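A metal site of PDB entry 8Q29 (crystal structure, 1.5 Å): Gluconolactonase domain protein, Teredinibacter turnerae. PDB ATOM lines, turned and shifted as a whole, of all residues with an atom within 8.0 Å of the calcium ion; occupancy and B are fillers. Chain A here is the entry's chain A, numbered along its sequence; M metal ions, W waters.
ND2 of Asn 56 sits at hydrogen-bond distance from O of Phe 11, 2.9 Å away.
The side-chain hydroxyl (OG1) of Thr 53 lies within hydrogen-bond range of the side-chain carboxylate (OD2) of Asp 226 (2.6 Å).
OD2 of Asp 225 lies close to N of Phe 52, 2.9 Å away.
The side-chain carboxylate of Glu 12 sits at hydrogen-bond distance from the backbone NH of Asn 55.
Of the 21 residues printed, 5 come within 4 Å of the calcium ion.
The nearest printed residue that does not touch the calcium ion is Asp 226 (4.4 Å).
The calcium ion is bound by OE2 of Glu 12, O of Asn 56, O of Gly 10, water W1, O of Thr 53, OD1 of Asp 225 and OD2 of Asp 225.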
ATOM      1  N   ASP A   9      23.958  23.479 -13.167  1.00  0.00           N
ATOM      2  CA  ASP A   9      22.592  23.992 -13.154  1.00  0.00           C
ATOM      3  C   ASP A   9      21.620  22.810 -13.167  1.00  0.00           C
ATOM      4  O   ASP A   9      21.674  22.001 -14.087  1.00  0.00           O
ATOM      5  CB  ASP A   9      22.350  24.939 -14.335  1.00  0.00           C
ATOM      6  CG  ASP A   9      21.115  25.824 -14.165  1.00  0.00           C
ATOM      7  OD1 ASP A   9      20.301  25.557 -13.265  1.00  0.00           O
ATOM      8  OD2 ASP A   9      21.028  26.794 -14.953  1.00  0.00           O
ATOM      9  N   GLY A  10      20.735  22.741 -12.158  1.00  0.00           N
ATOM     10  CA  GLY A  10      19.682  21.745 -12.054  1.00  0.00           C
ATOM     11  C   GLY A  10      18.298  22.307 -12.408  1.00  0.00           C
ATOM     12  O   GLY A  10      17.296  21.609 -12.276  1.00  0.00           O
ATOM     13  N   PHE A  11      18.235  23.604 -12.755  1.00  0.00           N
ATOM     14  CA  PHE A  11      17.012  24.299 -13.206  1.00  0.00           C
ATOM     15  C   PHE A  11      15.921  24.453 -12.137  1.00  0.00           C
ATOM     16  O   PHE A  11      14.777  24.723 -12.479  1.00  0.00           O
ATOM     17  CB  PHE A  11      16.472  23.650 -14.472  1.00  0.00           C
ATOM     18  CG  PHE A  11      17.514  23.513 -15.533  1.00  0.00           C
ATOM     19  CD1 PHE A  11      17.977  24.652 -16.205  1.00  0.00           C
ATOM     20  CD2 PHE A  11      18.138  22.315 -15.815  1.00  0.00           C
ATOM     21  CE1 PHE A  11      19.051  24.585 -17.082  1.00  0.00           C
ATOM     22  CE2 PHE A  11      19.217  22.275 -16.681  1.00  0.00           C
ATOM     23  CZ  PHE A  11      19.601  23.379 -17.364  1.00  0.00           C
ATOM     24  N   GLU A  12      16.282  24.311 -10.853  1.00  0.00           N
ATOM     25  CA  GLU A  12      15.309  24.269  -9.790  1.00  0.00           C
ATOM     26  C   GLU A  12      14.840  25.679  -9.454  1.00  0.00           C
ATOM     27  O   GLU A  12      13.771  25.806  -8.899  1.00  0.00           O
ATOM     28  CB  GLU A  12      15.877  23.559  -8.582  1.00  0.00           C
ATOM     29  CG  GLU A  12      16.221  22.105  -8.866  1.00  0.00           C
ATOM     30  CD  GLU A  12      15.034  21.234  -9.282  1.00  0.00           C
ATOM     31  OE1 GLU A  12      13.953  21.345  -8.608  1.00  0.00           O
ATOM     32  OE2 GLU A  12      15.174  20.450 -10.322  1.00  0.00           O
ATOM     33  N   SER A  13      15.605  26.726  -9.808  1.00  0.00           N
ATOM     34  CA  SER A  13      15.210  28.073  -9.405  1.00  0.00           C
ATOM     35  C   SER A  13      14.412  28.822 -10.477  1.00  0.00           C
ATOM     36  O   SER A  13      14.082  29.996 -10.293  1.00  0.00           O
ATOM     37  CB  SER A  13      16.420  28.872  -9.039  1.00  0.00           C
ATOM     38  OG  SER A  13      17.283  28.986 -10.146  1.00  0.00           O
ATOM     39  N   VAL A  46      12.037  25.336 -19.097  1.00  0.00           N
ATOM     40  CA  VAL A  46      12.002  24.523 -17.905  1.00  0.00           C
ATOM     41  C   VAL A  46      10.682  23.762 -17.823  1.00  0.00           C
ATOM     42  O   VAL A  46       9.593  24.290 -18.145  1.00  0.00           O
ATOM     43  CB  VAL A  46      12.267  25.425 -16.696  1.00  0.00           C
ATOM     44  CG1 VAL A  46      12.085  24.682 -15.371  1.00  0.00           C
ATOM     45  CG2 VAL A  46      13.690  25.928 -16.787  1.00  0.00           C
ATOM     46  N   ASP A  47      10.775  22.505 -17.374  1.00  0.00           N
ATOM     47  CA  ASP A  47       9.681  21.569 -17.367  1.00  0.00           C
ATOM     48  C   ASP A  47       9.745  20.747 -16.066  1.00  0.00           C
ATOM     49  O   ASP A  47      10.832  20.298 -15.695  1.00  0.00           O
ATOM     50  CB  ASP A  47       9.815  20.642 -18.586  1.00  0.00           C
ATOM     51  CG  ASP A  47       8.646  19.714 -18.875  1.00  0.00           C
ATOM     52  OD1 ASP A  47       7.751  19.625 -18.020  1.00  0.00           O
ATOM     53  OD2 ASP A  47       8.712  19.003 -19.899  1.00  0.00           O
ATOM     54  N   ARG A  50       9.296  15.906 -15.904  1.00  0.00           N
ATOM     55  CA  ARG A  50      10.370  14.943 -15.872  1.00  0.00           C
ATOM     56  C   ARG A  50      11.616  15.688 -15.393  1.00  0.00           C
ATOM     57  O   ARG A  50      11.805  16.879 -15.654  1.00  0.00           O
ATOM     58  CB  ARG A  50      10.448  14.430 -17.312  1.00  0.00           C
ATOM     59  CG  ARG A  50      11.747  13.881 -17.778  1.00  0.00           C
ATOM     60  CD  ARG A  50      11.669  13.052 -19.005  1.00  0.00           C
ATOM     61  NE  ARG A  50      10.724  11.989 -19.024  1.00  0.00           N
ATOM     62  CZ  ARG A  50       9.771  11.851 -19.914  1.00  0.00           C
ATOM     63  NH1 ARG A  50       9.666  12.668 -20.927  1.00  0.00           N
ATOM     64  NH2 ARG A  50       8.894  10.899 -19.783  1.00  0.00           N
ATOM     65  N   ALA A  51      12.422  14.996 -14.589  1.00  0.00           N
ATOM     66  CA  ALA A  51      13.673  15.523 -14.067  1.00  0.00           C
ATOM     67  C   ALA A  51      14.539  14.372 -13.582  1.00  0.00           C
ATOM     68  O   ALA A  51      14.047  13.294 -13.325  1.00  0.00           O
ATOM     69  CB  ALA A  51      13.408  16.541 -12.980  1.00  0.00           C
ATOM     70  N   PHE A  52      15.843  14.608 -13.490  1.00  0.00           N
ATOM     71  CA  PHE A  52      16.732  13.604 -12.918  1.00  0.00           C
ATOM     72  C   PHE A  52      16.938  13.877 -11.428  1.00  0.00           C
ATOM     73  O   PHE A  52      16.991  12.927 -10.623  1.00  0.00           O
ATOM     74  CB  PHE A  52      18.096  13.564 -13.599  1.00  0.00           C
ATOM     75  CG  PHE A  52      18.796  12.307 -13.206  1.00  0.00           C
ATOM     76  CD1 PHE A  52      18.440  11.094 -13.751  1.00  0.00           C
ATOM     77  CD2 PHE A  52      19.844  12.353 -12.324  1.00  0.00           C
ATOM     78  CE1 PHE A  52      19.031   9.911 -13.356  1.00  0.00           C
ATOM     79  CE2 PHE A  52      20.421  11.185 -11.906  1.00  0.00           C
ATOM     80  CZ  PHE A  52      20.038   9.970 -12.436  1.00  0.00           C
ATOM     81  N   THR A  53      17.087  15.125 -11.056  1.00  0.00           N
ATOM     82  CA  THR A  53      17.212  15.541  -9.684  1.00  0.00           C
ATOM     83  C   THR A  53      16.224  16.688  -9.435  1.00  0.00           C
ATOM     84  O   THR A  53      16.084  17.573 -10.284  1.00  0.00           O
ATOM     85  CB  THR A  53      18.641  15.972  -9.325  1.00  0.00           C
ATOM     86  OG1 THR A  53      19.530  15.039  -9.903  1.00  0.00           O
ATOM     87  CG2 THR A  53      18.851  15.976  -7.826  1.00  0.00           C
ATOM     88  N   GLY A  54      15.615  16.722  -8.270  1.00  0.00           N
ATOM     89  CA  GLY A  54      14.629  17.763  -7.981  1.00  0.00           C
ATOM     90  C   GLY A  54      13.412  17.627  -8.890  1.00  0.00           C
ATOM     91  O   GLY A  54      13.068  16.527  -9.341  1.00  0.00           O
ATOM     92  N   ASN A  55      12.711  18.760  -9.094  1.00  0.00           N
ATOM     93  CA  ASN A  55      11.461  18.764  -9.851  1.00  0.00           C
ATOM     94  C   ASN A  55      11.618  19.120 -11.319  1.00  0.00           C
ATOM     95  O   ASN A  55      10.747  18.745 -12.101  1.00  0.00           O
ATOM     96  CB  ASN A  55      10.472  19.755  -9.236  1.00  0.00           C
ATOM     97  CG  ASN A  55      10.227  19.390  -7.787  1.00  0.00           C
ATOM     98  OD1 ASN A  55      10.445  20.167  -6.885  1.00  0.00           O
ATOM     99  ND2 ASN A  55       9.864  18.151  -7.544  1.00  0.00           N
ATOM    100  N   ASN A  56      12.693  19.825 -11.654  1.00  0.00           N
ATOM    101  CA  ASN A  56      12.735  20.524 -12.946  1.00  0.00           C
ATOM    102  C   ASN A  56      13.884  19.972 -13.831  1.00  0.00           C
ATOM    103  O   ASN A  56      14.987  19.676 -13.358  1.00  0.00           O
ATOM    104  CB  ASN A  56      12.967  22.013 -12.762  1.00  0.00           C
ATOM    105  CG  ASN A  56      11.825  22.764 -12.112  1.00  0.00           C
ATOM    106  OD1 ASN A  56      10.728  22.213 -11.947  1.00  0.00           O
ATOM    107  ND2 ASN A  56      12.068  24.022 -11.779  1.00  0.00           N
ATOM    108  N   SER A  57      13.650  19.983 -15.148  1.00  0.00           N
ATOM    109  CA  SER A  57      14.669  19.842 -16.138  1.00  0.00           C
ATOM    110  C   SER A  57      14.449  20.949 -17.159  1.00  0.00           C
ATOM    111  O   SER A  57      13.485  21.705 -17.065  1.00  0.00           O
ATOM    112  CB  SER A  57      14.584  18.495 -16.796  1.00  0.00           C
ATOM    113  OG  SER A  57      13.311  18.312 -17.388  1.00  0.00           O
ATOM    114  N   VAL A  58      15.336  21.000 -18.154  1.00  0.00           N
ATOM    115  CA  VAL A  58      15.108  21.788 -19.356  1.00  0.00           C
ATOM    116  C   VAL A  58      14.610  20.861 -20.457  1.00  0.00           C
ATOM    117  O   VAL A  58      15.222  19.832 -20.715  1.00  0.00           O
ATOM    118  CB  VAL A  58      16.323  22.631 -19.793  1.00  0.00           C
ATOM    119  CG1 VAL A  58      17.584  21.809 -20.041  1.00  0.00           C
ATOM    120  CG2 VAL A  58      16.006  23.473 -21.029  1.00  0.00           C
ATOM    121  N   TRP A 154      17.340   7.958 -18.841  1.00  0.00           N
ATOM    122  CA  TRP A 154      18.350   8.952 -18.508  1.00  0.00           C
ATOM    123  C   TRP A 154      19.748   8.422 -18.751  1.00  0.00           C
ATOM    124  O   TRP A 154      20.075   7.313 -18.363  1.00  0.00           O
ATOM    125  CB  TRP A 154      18.228   9.379 -17.054  1.00  0.00           C
ATOM    126  CG  TRP A 154      17.018  10.236 -16.778  1.00  0.00           C
ATOM    127  CD1 TRP A 154      15.831   9.853 -16.245  1.00  0.00           C
ATOM    128  CD2 TRP A 154      16.905  11.651 -17.070  1.00  0.00           C
ATOM    129  NE1 TRP A 154      15.006  10.917 -16.104  1.00  0.00           N
ATOM    130  CE2 TRP A 154      15.631  12.049 -16.624  1.00  0.00           C
ATOM    131  CE3 TRP A 154      17.766  12.581 -17.659  1.00  0.00           C
ATOM    132  CZ2 TRP A 154      15.162  13.343 -16.815  1.00  0.00           C
ATOM    133  CZ3 TRP A 154      17.314  13.864 -17.780  1.00  0.00           C
ATOM    134  CH2 TRP A 154      16.049  14.239 -17.335  1.00  0.00           C
ATOM    135  N   MET A 224      17.074  17.703 -20.332  1.00  0.00           N
ATOM    136  CA  MET A 224      18.373  17.614 -19.681  1.00  0.00           C
ATOM    137  C   MET A 224      18.296  18.182 -18.294  1.00  0.00           C
ATOM    138  O   MET A 224      17.507  19.050 -17.994  1.00  0.00           O
ATOM    139  CB  MET A 224      19.468  18.357 -20.476  1.00  0.00           C
ATOM    140  CG  MET A 224      19.702  17.788 -21.853  1.00  0.00           C
ATOM    141  SD  MET A 224      21.166  18.541 -22.624  1.00  0.00           S
ATOM    142  CE  MET A 224      20.936  17.923 -24.304  1.00  0.00           C
ATOM    143  N   ASP A 225      19.133  17.627 -17.410  1.00  0.00           N
ATOM    144  CA  ASP A 225      19.196  18.069 -16.045  1.00  0.00           C
ATOM    145  C   ASP A 225      20.648  18.006 -15.574  1.00  0.00           C
ATOM    146  O   ASP A 225      21.488  17.349 -16.181  1.00  0.00           O
ATOM    147  CB  ASP A 225      18.260  17.217 -15.168  1.00  0.00           C
ATOM    148  CG  ASP A 225      17.785  17.867 -13.902  1.00  0.00           C
ATOM    149  OD1 ASP A 225      18.212  19.003 -13.622  1.00  0.00           O
ATOM    150  OD2 ASP A 225      16.988  17.254 -13.156  1.00  0.00           O
ATOM    151  N   ASP A 226      20.925  18.747 -14.511  1.00  0.00           N
ATOM    152  CA  ASP A 226      22.228  18.690 -13.858  1.00  0.00           C
ATOM    153  C   ASP A 226      23.357  18.927 -14.852  1.00  0.00           C
ATOM    154  O   ASP A 226      24.299  18.135 -14.982  1.00  0.00           O
ATOM    155  CB  ASP A 226      22.378  17.402 -13.053  1.00  0.00           C
ATOM    156  CG  ASP A 226      21.240  17.220 -12.109  1.00  0.00           C
ATOM    157  OD1 ASP A 226      20.904  18.217 -11.455  1.00  0.00           O
ATOM    158  OD2 ASP A 226      20.714  16.054 -12.043  1.00  0.00           O
ATOM    159  N   ILE A 227      23.192  19.992 -15.646  1.00  0.00           N
ATOM    160  CA  ILE A 227      24.189  20.360 -16.629  1.00  0.00           C
ATOM    161  C   ILE A 227      25.391  20.951 -15.953  1.00  0.00           C
ATOM    162  O   ILE A 227      25.271  21.747 -15.002  1.00  0.00           O
ATOM    163  CB  ILE A 227      23.558  21.340 -17.641  1.00  0.00           C
ATOM    164  CG1 ILE A 227      22.441  20.629 -18.436  1.00  0.00           C
ATOM    165  CG2 ILE A 227      24.623  21.901 -18.537  1.00  0.00           C
ATOM    166  CD1 ILE A 227      21.848  21.448 -19.577  1.00  0.00           C
HETATM  167 CA    CA M   1      16.664  19.392 -11.745  1.00  0.00          CA
HETATM  168  O   HOH W   1      18.586  19.292 -10.359  1.00  0.00           O
